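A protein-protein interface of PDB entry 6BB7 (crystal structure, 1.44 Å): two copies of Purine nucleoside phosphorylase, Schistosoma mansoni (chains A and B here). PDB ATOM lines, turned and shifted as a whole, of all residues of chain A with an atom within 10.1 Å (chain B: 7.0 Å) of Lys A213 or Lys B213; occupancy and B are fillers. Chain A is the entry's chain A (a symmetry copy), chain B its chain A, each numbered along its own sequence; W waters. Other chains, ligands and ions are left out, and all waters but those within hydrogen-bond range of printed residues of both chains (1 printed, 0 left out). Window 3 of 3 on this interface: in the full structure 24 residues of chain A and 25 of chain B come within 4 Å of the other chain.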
ATOM      1  N   ILE A 122      10.806 -11.158 -33.465  1.00  0.00           N
ATOM      2  CA  ILE A 122       9.614 -11.812 -33.997  1.00  0.00           C
ATOM      3  C   ILE A 122       8.668 -10.796 -34.662  1.00  0.00           C
ATOM      4  O   ILE A 122       8.253 -10.984 -35.804  1.00  0.00           O
ATOM      5  CB  ILE A 122       8.888 -12.648 -32.908  1.00  0.00           C
ATOM      6  CG1 ILE A 122       9.803 -13.737 -32.284  1.00  0.00           C
ATOM      7  CG2 ILE A 122       7.589 -13.278 -33.458  1.00  0.00           C
ATOM      8  CD1 ILE A 122      10.244 -14.827 -33.224  1.00  0.00           C
ATOM      9  N   ASN A 123       8.319  -9.722 -33.949  1.00  0.00           N
ATOM     10  CA  ASN A 123       7.480  -8.659 -34.499  1.00  0.00           C
ATOM     11  C   ASN A 123       8.081  -8.125 -35.794  1.00  0.00           C
ATOM     12  O   ASN A 123       9.290  -7.892 -35.883  1.00  0.00           O
ATOM     13  CB  ASN A 123       7.420  -7.517 -33.469  1.00  0.00           C
ATOM     14  CG  ASN A 123       6.385  -6.456 -33.811  1.00  0.00           C
ATOM     15  OD1 ASN A 123       6.462  -5.812 -34.854  1.00  0.00           O
ATOM     16  ND2 ASN A 123       5.405  -6.273 -32.924  1.00  0.00           N
ATOM     17  N   ARG A 124       7.220  -7.891 -36.788  1.00  0.00           N
ATOM     18  CA  ARG A 124       7.710  -7.468 -38.097  1.00  0.00           C
ATOM     19  C   ARG A 124       8.342  -6.079 -38.085  1.00  0.00           C
ATOM     20  O   ARG A 124       9.101  -5.762 -39.000  1.00  0.00           O
ATOM     21  CB  ARG A 124       6.601  -7.592 -39.149  1.00  0.00           C
ATOM     22  CG  ARG A 124       6.423  -9.049 -39.602  1.00  0.00           C
ATOM     23  CD  ARG A 124       5.206  -9.245 -40.490  1.00  0.00           C
ATOM     24  NE  ARG A 124       4.934 -10.657 -40.771  1.00  0.00           N
ATOM     25  CZ  ARG A 124       5.648 -11.421 -41.597  1.00  0.00           C
ATOM     26  NH1 ARG A 124       6.718 -10.932 -42.224  1.00  0.00           N
ATOM     27  NH2 ARG A 124       5.299 -12.691 -41.784  1.00  0.00           N
ATOM     28  N   ILE A 138       6.514 -14.199 -21.675  1.00  0.00           N
ATOM     29  CA  ILE A 138       5.896 -15.524 -21.751  1.00  0.00           C
ATOM     30  C   ILE A 138       6.974 -16.551 -21.372  1.00  0.00           C
ATOM     31  O   ILE A 138       7.962 -16.747 -22.096  1.00  0.00           O
ATOM     32  CB  ILE A 138       5.281 -15.814 -23.126  1.00  0.00           C
ATOM     33  CG1 ILE A 138       4.119 -14.838 -23.405  1.00  0.00           C
ATOM     34  CG2 ILE A 138       4.796 -17.273 -23.215  1.00  0.00           C
ATOM     35  CD1 ILE A 138       3.619 -14.879 -24.822  1.00  0.00           C
ATOM     36  N   PHE A 140       8.013 -19.998 -20.965  1.00  0.00           N
ATOM     37  CA  PHE A 140       7.764 -21.405 -21.301  1.00  0.00           C
ATOM     38  C   PHE A 140       8.323 -22.351 -20.243  1.00  0.00           C
ATOM     39  O   PHE A 140       7.603 -23.310 -19.869  1.00  0.00           O
ATOM     40  CB  PHE A 140       8.245 -21.727 -22.731  1.00  0.00           C
ATOM     41  CG  PHE A 140       7.387 -21.092 -23.801  1.00  0.00           C
ATOM     42  CD1 PHE A 140       6.120 -21.577 -24.076  1.00  0.00           C
ATOM     43  CD2 PHE A 140       7.849 -20.000 -24.514  1.00  0.00           C
ATOM     44  CE1 PHE A 140       5.319 -20.974 -25.060  1.00  0.00           C
ATOM     45  CE2 PHE A 140       7.043 -19.400 -25.484  1.00  0.00           C
ATOM     46  CZ  PHE A 140       5.799 -19.884 -25.757  1.00  0.00           C
ATOM     47  N   VAL A 193       6.906  -7.767 -25.748  1.00  0.00           N
ATOM     48  CA  VAL A 193       6.793  -8.970 -24.913  1.00  0.00           C
ATOM     49  C   VAL A 193       7.901  -9.967 -25.268  1.00  0.00           C
ATOM     50  O   VAL A 193       8.077 -10.324 -26.445  1.00  0.00           O
ATOM     51  CB  VAL A 193       5.417  -9.616 -25.127  1.00  0.00           C
ATOM     52  CG1 VAL A 193       5.332 -10.950 -24.389  1.00  0.00           C
ATOM     53  CG2 VAL A 193       4.291  -8.658 -24.697  1.00  0.00           C
ATOM     54  N   PRO A 205      12.808 -22.369 -37.327  1.00  0.00           N
ATOM     55  CA  PRO A 205      11.884 -21.581 -38.177  1.00  0.00           C
ATOM     56  C   PRO A 205      10.428 -21.785 -37.792  1.00  0.00           C
ATOM     57  O   PRO A 205       9.664 -20.815 -37.705  1.00  0.00           O
ATOM     58  CB  PRO A 205      12.187 -22.077 -39.594  1.00  0.00           C
ATOM     59  CG  PRO A 205      13.612 -22.554 -39.534  1.00  0.00           C
ATOM     60  CD  PRO A 205      13.849 -23.050 -38.132  1.00  0.00           C
ATOM     61  N   ASP A 206      10.017 -23.031 -37.523  1.00  0.00           N
ATOM     62  CA  ASP A 206       8.631 -23.277 -37.164  1.00  0.00           C
ATOM     63  C   ASP A 206       8.299 -22.834 -35.750  1.00  0.00           C
ATOM     64  O   ASP A 206       7.167 -22.415 -35.495  1.00  0.00           O
ATOM     65  CB  ASP A 206       8.286 -24.743 -37.427  1.00  0.00           C
ATOM     66  CG  ASP A 206       8.393 -25.079 -38.894  1.00  0.00           C
ATOM     67  OD1 ASP A 206       7.524 -24.617 -39.687  1.00  0.00           O
ATOM     68  OD2 ASP A 206       9.373 -25.754 -39.290  1.00  0.00           O
ATOM     69  N   GLU A 207       9.245 -22.910 -34.800  1.00  0.00           N
ATOM     70  CA  GLU A 207       9.022 -22.295 -33.497  1.00  0.00           C
ATOM     71  C   GLU A 207       8.816 -20.777 -33.620  1.00  0.00           C
ATOM     72  O   GLU A 207       7.961 -20.206 -32.934  1.00  0.00           O
ATOM     73  CB  GLU A 207      10.174 -22.635 -32.533  1.00  0.00           C
ATOM     74  CG  GLU A 207      10.201 -24.138 -32.143  1.00  0.00           C
ATOM     75  CD  GLU A 207      11.552 -24.646 -31.659  1.00  0.00           C
ATOM     76  OE1 GLU A 207      12.533 -23.870 -31.528  1.00  0.00           O
ATOM     77  OE2 GLU A 207      11.629 -25.871 -31.389  1.00  0.00           O
ATOM     78  N   SER A 208       9.592 -20.117 -34.471  1.00  0.00           N
ATOM     79  CA  SER A 208       9.435 -18.676 -34.683  1.00  0.00           C
ATOM     80  C   SER A 208       8.035 -18.346 -35.183  1.00  0.00           C
ATOM     81  O   SER A 208       7.383 -17.428 -34.657  1.00  0.00           O
ATOM     82  CB  SER A 208      10.488 -18.177 -35.671  1.00  0.00           C
ATOM     83  OG  SER A 208      11.784 -18.307 -35.108  1.00  0.00           O
ATOM     84  N   ASN A 209       7.547 -19.108 -36.164  1.00  0.00           N
ATOM     85  CA  ASN A 209       6.197 -18.898 -36.697  1.00  0.00           C
ATOM     86  C   ASN A 209       5.145 -19.089 -35.615  1.00  0.00           C
ATOM     87  O   ASN A 209       4.160 -18.336 -35.553  1.00  0.00           O
ATOM     88  CB  ASN A 209       5.951 -19.835 -37.881  1.00  0.00           C
ATOM     89  CG  ASN A 209       6.722 -19.422 -39.128  1.00  0.00           C
ATOM     90  OD1 ASN A 209       7.086 -18.251 -39.304  1.00  0.00           O
ATOM     91  ND2 ASN A 209       6.976 -20.387 -40.004  1.00  0.00           N
ATOM     92  N   MET A 210       5.341 -20.071 -34.731  1.00  0.00           N
ATOM     93  CA  MET A 210       4.413 -20.264 -33.626  1.00  0.00           C
ATOM     94  C   MET A 210       4.406 -19.043 -32.709  1.00  0.00           C
ATOM     95  O   MET A 210       3.336 -18.570 -32.295  1.00  0.00           O
ATOM     96  CB  MET A 210       4.784 -21.521 -32.844  1.00  0.00           C
ATOM     97  CG  MET A 210       3.846 -21.802 -31.668  1.00  0.00           C
ATOM     98  SD  MET A 210       4.311 -23.220 -30.662  1.00  0.00           S
ATOM     99  CE  MET A 210       5.763 -22.647 -29.895  1.00  0.00           C
ATOM    100  N   LEU A 211       5.594 -18.522 -32.371  1.00  0.00           N
ATOM    101  CA  LEU A 211       5.687 -17.395 -31.436  1.00  0.00           C
ATOM    102  C   LEU A 211       5.009 -16.146 -31.978  1.00  0.00           C
ATOM    103  O   LEU A 211       4.427 -15.364 -31.206  1.00  0.00           O
ATOM    104  CB  LEU A 211       7.153 -17.118 -31.103  1.00  0.00           C
ATOM    105  CG  LEU A 211       7.895 -18.227 -30.355  1.00  0.00           C
ATOM    106  CD1 LEU A 211       9.364 -17.862 -30.219  1.00  0.00           C
ATOM    107  CD2 LEU A 211       7.277 -18.504 -28.991  1.00  0.00           C
ATOM    108  N   LEU A 212       5.068 -15.936 -33.285  1.00  0.00           N
ATOM    109  CA  LEU A 212       4.341 -14.823 -33.883  1.00  0.00           C
ATOM    110  C   LEU A 212       2.849 -14.943 -33.595  1.00  0.00           C
ATOM    111  O   LEU A 212       2.206 -13.968 -33.187  1.00  0.00           O
ATOM    112  CB  LEU A 212       4.609 -14.767 -35.382  1.00  0.00           C
ATOM    113  CG  LEU A 212       3.939 -13.632 -36.156  1.00  0.00           C
ATOM    114  CD1 LEU A 212       4.483 -12.284 -35.698  1.00  0.00           C
ATOM    115  CD2 LEU A 212       4.174 -13.826 -37.641  1.00  0.00           C
ATOM    116  N   LYS A 213       2.288 -16.145 -33.777  1.00  0.00           N
ATOM    117  CA  LYS A 213       0.857 -16.371 -33.533  1.00  0.00           C
ATOM    118  C   LYS A 213       0.471 -16.127 -32.072  1.00  0.00           C
ATOM    119  O   LYS A 213      -0.690 -15.785 -31.792  1.00  0.00           O
ATOM    120  CB  LYS A 213       0.483 -17.818 -33.916  1.00  0.00           C
ATOM    121  CG  LYS A 213       0.569 -18.197 -35.400  1.00  0.00           C
ATOM    122  CD  LYS A 213       0.292 -19.712 -35.599  1.00  0.00           C
ATOM    123  CE  LYS A 213       0.169 -20.118 -37.062  1.00  0.00           C
ATOM    124  NZ  LYS A 213       1.411 -20.725 -37.599  1.00  0.00           N
ATOM    125  N   LEU A 214       1.401 -16.311 -31.132  1.00  0.00           N
ATOM    126  CA  LEU A 214       1.115 -16.284 -29.698  1.00  0.00           C
ATOM    127  C   LEU A 214       1.327 -14.918 -29.060  1.00  0.00           C
ATOM    128  O   LEU A 214       1.221 -14.797 -27.831  1.00  0.00           O
ATOM    129  CB  LEU A 214       1.980 -17.299 -28.968  1.00  0.00           C
ATOM    130  CG  LEU A 214       1.736 -18.763 -29.325  1.00  0.00           C
ATOM    131  CD1 LEU A 214       2.679 -19.652 -28.573  1.00  0.00           C
ATOM    132  CD2 LEU A 214       0.308 -19.128 -29.023  1.00  0.00           C
ATOM    133  N   GLY A 215       1.638 -13.903 -29.852  1.00  0.00           N
ATOM    134  CA  GLY A 215       1.788 -12.571 -29.316  1.00  0.00           C
ATOM    135  C   GLY A 215       3.163 -12.225 -28.787  1.00  0.00           C
ATOM    136  O   GLY A 215       3.294 -11.280 -28.003  1.00  0.00           O
ATOM    137  N   CYS A 216       4.196 -12.958 -29.179  1.00  0.00           N
ATOM    138  CA  CYS A 216       5.557 -12.668 -28.747  1.00  0.00           C
ATOM    139  C   CYS A 216       6.207 -11.680 -29.710  1.00  0.00           C
ATOM    140  O   CYS A 216       6.062 -11.791 -30.927  1.00  0.00           O
ATOM    141  CB  CYS A 216       6.403 -13.949 -28.675  1.00  0.00           C
ATOM    142  SG  CYS A 216       5.693 -15.239 -27.606  1.00  0.00           S
ATOM    143  N   ASP A 217       6.924 -10.701 -29.156  1.00  0.00           N
ATOM    144  CA  ASP A 217       7.658  -9.741 -29.971  1.00  0.00           C
ATOM    145  C   ASP A 217       9.140 -10.082 -30.144  1.00  0.00           C
ATOM    146  O   ASP A 217       9.706  -9.764 -31.199  1.00  0.00           O
ATOM    147  CB  ASP A 217       7.535  -8.343 -29.361  1.00  0.00           C
ATOM    148  CG  ASP A 217       6.076  -7.858 -29.335  1.00  0.00           C
ATOM    149  OD1 ASP A 217       5.471  -7.795 -30.428  1.00  0.00           O
ATOM    150  OD2 ASP A 217       5.550  -7.562 -28.242  1.00  0.00           O
ATOM    151  N   ILE A 248      11.521 -14.265 -38.236  1.00  0.00           N
ATOM    152  CA  ILE A 248      10.431 -14.491 -39.187  1.00  0.00           C
ATOM    153  C   ILE A 248      10.896 -14.209 -40.622  1.00  0.00           C
ATOM    154  O   ILE A 248      10.622 -14.983 -41.548  1.00  0.00           O
ATOM    155  CB  ILE A 248       9.191 -13.654 -38.791  1.00  0.00           C
ATOM    156  CG1 ILE A 248       8.600 -14.100 -37.449  1.00  0.00           C
ATOM    157  CG2 ILE A 248       8.125 -13.692 -39.884  1.00  0.00           C
ATOM    158  CD1 ILE A 248       7.985 -15.504 -37.455  1.00  0.00           C
ATOM    159  N   GLU A 252      11.359 -16.956 -43.874  1.00  0.00           N
ATOM    160  CA  GLU A 252      10.794 -16.761 -45.206  1.00  0.00           C
ATOM    161  C   GLU A 252      11.862 -16.750 -46.309  1.00  0.00           C
ATOM    162  O   GLU A 252      11.549 -17.081 -47.464  1.00  0.00           O
ATOM    163  CB  GLU A 252       9.904 -15.500 -45.210  1.00  0.00           C
ATOM    164  CG  GLU A 252       8.746 -15.646 -44.215  1.00  0.00           C
ATOM    165  CD  GLU A 252       7.863 -14.411 -44.024  1.00  0.00           C
ATOM    166  OE1 GLU A 252       6.738 -14.581 -43.497  1.00  0.00           O
ATOM    167  OE2 GLU A 252       8.277 -13.283 -44.364  1.00  0.00           O
ATOM    168  N   ILE B 122      -9.976 -17.575 -17.422  1.00  0.00           N
ATOM    169  CA  ILE B 122      -9.562 -17.079 -18.730  1.00  0.00           C
ATOM    170  C   ILE B 122     -10.778 -16.753 -19.616  1.00  0.00           C
ATOM    171  O   ILE B 122     -10.873 -15.658 -20.167  1.00  0.00           O
ATOM    172  CB  ILE B 122      -8.587 -18.064 -19.432  1.00  0.00           C
ATOM    173  CG1 ILE B 122      -7.311 -18.341 -18.590  1.00  0.00           C
ATOM    174  CG2 ILE B 122      -8.210 -17.569 -20.846  1.00  0.00           C
ATOM    175  CD1 ILE B 122      -6.406 -17.157 -18.380  1.00  0.00           C
ATOM    176  N   ASP B 206       0.657 -11.388 -20.011  1.00  0.00           N
ATOM    177  CA  ASP B 206       0.843 -11.863 -21.371  1.00  0.00           C
ATOM    178  C   ASP B 206       0.677 -13.367 -21.499  1.00  0.00           C
ATOM    179  O   ASP B 206       0.218 -13.840 -22.542  1.00  0.00           O
ATOM    180  CB  ASP B 206       2.183 -11.362 -21.910  1.00  0.00           C
ATOM    181  CG  ASP B 206       2.213  -9.855 -21.997  1.00  0.00           C
ATOM    182  OD1 ASP B 206       1.516  -9.285 -22.884  1.00  0.00           O
ATOM    183  OD2 ASP B 206       2.878  -9.214 -21.149  1.00  0.00           O
ATOM    184  N   SER B 208      -1.579 -14.983 -19.772  1.00  0.00           N
ATOM    185  CA  SER B 208      -3.041 -15.081 -19.780  1.00  0.00           C
ATOM    186  C   SER B 208      -3.596 -14.837 -21.177  1.00  0.00           C
ATOM    187  O   SER B 208      -4.441 -15.611 -21.659  1.00  0.00           O
ATOM    188  CB  SER B 208      -3.635 -14.087 -18.786  1.00  0.00           C
ATOM    189  OG  SER B 208      -3.270 -14.445 -17.462  1.00  0.00           O
ATOM    190  N   ASN B 209      -3.106 -13.794 -21.850  1.00  0.00           N
ATOM    191  CA  ASN B 209      -3.548 -13.487 -23.215  1.00  0.00           C
ATOM    192  C   ASN B 209      -3.233 -14.634 -24.163  1.00  0.00           C
ATOM    193  O   ASN B 209      -4.044 -14.967 -25.042  1.00  0.00           O
ATOM    194  CB  ASN B 209      -2.906 -12.183 -23.691  1.00  0.00           C
ATOM    195  CG  ASN B 209      -3.498 -10.954 -23.011  1.00  0.00           C
ATOM    196  OD1 ASN B 209      -4.641 -10.968 -22.533  1.00  0.00           O
ATOM    197  ND2 ASN B 209      -2.718  -9.880 -22.964  1.00  0.00           N
ATOM    198  N   MET B 210      -2.074 -15.275 -23.992  1.00  0.00           N
ATOM    199  CA  MET B 210      -1.740 -16.429 -24.816  1.00  0.00           C
ATOM    200  C   MET B 210      -2.737 -17.561 -24.585  1.00  0.00           C
ATOM    201  O   MET B 210      -3.210 -18.193 -25.543  1.00  0.00           O
ATOM    202  CB  MET B 210      -0.318 -16.894 -24.515  1.00  0.00           C
ATOM    203  CG  MET B 210       0.114 -18.100 -25.352  1.00  0.00           C
ATOM    204  SD  MET B 210       1.749 -18.740 -24.953  1.00  0.00           S
ATOM    205  CE  MET B 210       1.486 -19.415 -23.372  1.00  0.00           C
ATOM    206  N   LEU B 211      -3.063 -17.843 -23.315  1.00  0.00           N
ATOM    207  CA  LEU B 211      -3.955 -18.963 -22.995  1.00  0.00           C
ATOM    208  C   LEU B 211      -5.348 -18.767 -23.574  1.00  0.00           C
ATOM    209  O   LEU B 211      -6.001 -19.746 -23.978  1.00  0.00           O
ATOM    210  CB  LEU B 211      -4.019 -19.157 -21.479  1.00  0.00           C
ATOM    211  CG  LEU B 211      -2.714 -19.572 -20.798  1.00  0.00           C
ATOM    212  CD1 LEU B 211      -2.904 -19.591 -19.290  1.00  0.00           C
ATOM    213  CD2 LEU B 211      -2.216 -20.921 -21.298  1.00  0.00           C
ATOM    214  N   LEU B 212      -5.821 -17.531 -23.628  1.00  0.00           N
ATOM    215  CA  LEU B 212      -7.097 -17.261 -24.278  1.00  0.00           C
ATOM    216  C   LEU B 212      -7.058 -17.705 -25.736  1.00  0.00           C
ATOM    217  O   LEU B 212      -7.981 -18.375 -26.215  1.00  0.00           O
ATOM    218  CB  LEU B 212      -7.440 -15.781 -24.164  1.00  0.00           C
ATOM    219  CG  LEU B 212      -8.770 -15.337 -24.774  1.00  0.00           C
ATOM    220  CD1 LEU B 212      -9.935 -15.979 -24.032  1.00  0.00           C
ATOM    221  CD2 LEU B 212      -8.870 -13.825 -24.719  1.00  0.00           C
ATOM    222  N   LYS B 213      -5.978 -17.362 -26.449  1.00  0.00           N
ATOM    223  CA  LYS B 213      -5.840 -17.735 -27.864  1.00  0.00           C
ATOM    224  C   LYS B 213      -5.808 -19.252 -28.064  1.00  0.00           C
ATOM    225  O   LYS B 213      -6.190 -19.737 -29.142  1.00  0.00           O
ATOM    226  CB  LYS B 213      -4.547 -17.124 -28.442  1.00  0.00           C
ATOM    227  CG  LYS B 213      -4.481 -15.595 -28.556  1.00  0.00           C
ATOM    228  CD  LYS B 213      -3.074 -15.138 -29.027  1.00  0.00           C
ATOM    229  CE  LYS B 213      -2.997 -13.651 -29.349  1.00  0.00           C
ATOM    230  NZ  LYS B 213      -2.403 -12.853 -28.249  1.00  0.00           N
ATOM    231  N   LEU B 214      -5.346 -20.013 -27.069  1.00  0.00           N
ATOM    232  CA  LEU B 214      -5.097 -21.448 -27.199  1.00  0.00           C
ATOM    233  C   LEU B 214      -6.274 -22.311 -26.763  1.00  0.00           C
ATOM    234  O   LEU B 214      -6.144 -23.542 -26.726  1.00  0.00           O
ATOM    235  CB  LEU B 214      -3.876 -21.848 -26.387  1.00  0.00           C
ATOM    236  CG  LEU B 214      -2.549 -21.243 -26.837  1.00  0.00           C
ATOM    237  CD1 LEU B 214      -1.438 -21.680 -25.930  1.00  0.00           C
ATOM    238  CD2 LEU B 214      -2.263 -21.644 -28.257  1.00  0.00           C
ATOM    239  N   GLY B 215      -7.399 -21.702 -26.420  1.00  0.00           N
ATOM    240  CA  GLY B 215      -8.569 -22.467 -26.061  1.00  0.00           C
ATOM    241  C   GLY B 215      -8.667 -22.876 -24.607  1.00  0.00           C
ATOM    242  O   GLY B 215      -9.411 -23.808 -24.285  1.00  0.00           O
ATOM    243  N   CYS B 216      -7.940 -22.220 -23.714  1.00  0.00           N
ATOM    244  CA  CYS B 216      -8.005 -22.526 -22.290  1.00  0.00           C
ATOM    245  C   CYS B 216      -9.108 -21.703 -21.634  1.00  0.00           C
ATOM    246  O   CYS B 216      -9.269 -20.515 -21.917  1.00  0.00           O
ATOM    247  CB  CYS B 216      -6.665 -22.236 -21.597  1.00  0.00           C
ATOM    248  SG  CYS B 216      -5.251 -23.111 -22.337  1.00  0.00           S
ATOM    249  N   ILE B 248      -7.884 -12.234 -17.576  1.00  0.00           N
ATOM    250  CA  ILE B 248      -7.965 -11.402 -18.778  1.00  0.00           C
ATOM    251  C   ILE B 248      -8.497 -10.005 -18.435  1.00  0.00           C
ATOM    252  O   ILE B 248      -7.964  -8.986 -18.893  1.00  0.00           O
ATOM    253  CB  ILE B 248      -8.813 -12.108 -19.863  1.00  0.00           C
ATOM    254  CG1 ILE B 248      -8.152 -13.400 -20.360  1.00  0.00           C
ATOM    255  CG2 ILE B 248      -9.104 -11.173 -21.035  1.00  0.00           C
ATOM    256  CD1 ILE B 248      -6.843 -13.194 -21.131  1.00  0.00           C
HETATM  257  O   HOH W   1       0.229 -12.974 -25.443  1.00  0.00           O
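The side-chain carboxylate (OD2) of Asp A217 is in hydrogen-bond range of the backbone NH (N) of Val A193.
Ile A138 touches Met B210. Asp B206 touches Val A193 (OD1 to CG2, 3.4 Å). Lys A213 touches Lys B213. CG of Met B210 touches CD2 of Leu A214, 3.8 Å away. CD2 of Leu B214 touches CD2 of Leu A214 (3.7 Å).
Of the printed residues of chain B, Ile A138 touches Met B210. Of the printed residues of chain B, Val A193 touches Asp B206. Lys A213 touches just one residue of chain B: Lys B213 (3.7 Å). Of the printed residues of chain B, Leu A214 touches Met B210 and Leu B214. Asp A217 touches none of the printed residues of chain B. Ile A248 touches none of the printed residues of chain B. Printed residues of chain A within 4 Å of Asp B206: Val A193. Of the printed residues of chain A, Met B210 touches Ile A138 (3.8 Å) and Leu A214 (3.8 Å). No residue of chain A comes within 4 Å of Leu B212. Printed residues of chain A within 4 Å of Lys B213: Lys A213 (3.7 Å).
Of the 21 printed residues of chain A, 4 touch a printed residue of chain B. Printed residues of chain A that touch a printed residue of chain B: Ile A138, Val A193, Lys A213 and Leu A214. Of the 12 printed residues of chain B, 4 touch a printed residue of chain A. Printed residues of chain B that touch a printed residue of chain A: Asp B206, Met B210, Lys B213 and Leu B214. Hydrophobic or aromatic side chains of chain B that line the printed part of chain A: Met B210 and Leu B214.
Lys A213 touches its own counterpart, Lys B213. Leu A214 touches Met B210, but with the chains exchanged Met A210 does not touch Leu B214 (7.0 Å). Leu A214 touches its own counterpart, Leu B214. Positions printed for both chains: 122, 206, 208, 209, 210, 211, 212, 213, 214, 215, 216 and 248. Of the 5 pairs that touch across the chains among the printed residues, 2 have their exchanged pair printed and touching as well.
Water W1 lies within hydrogen-bond range of O of Asp B206 and O of Leu A214.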
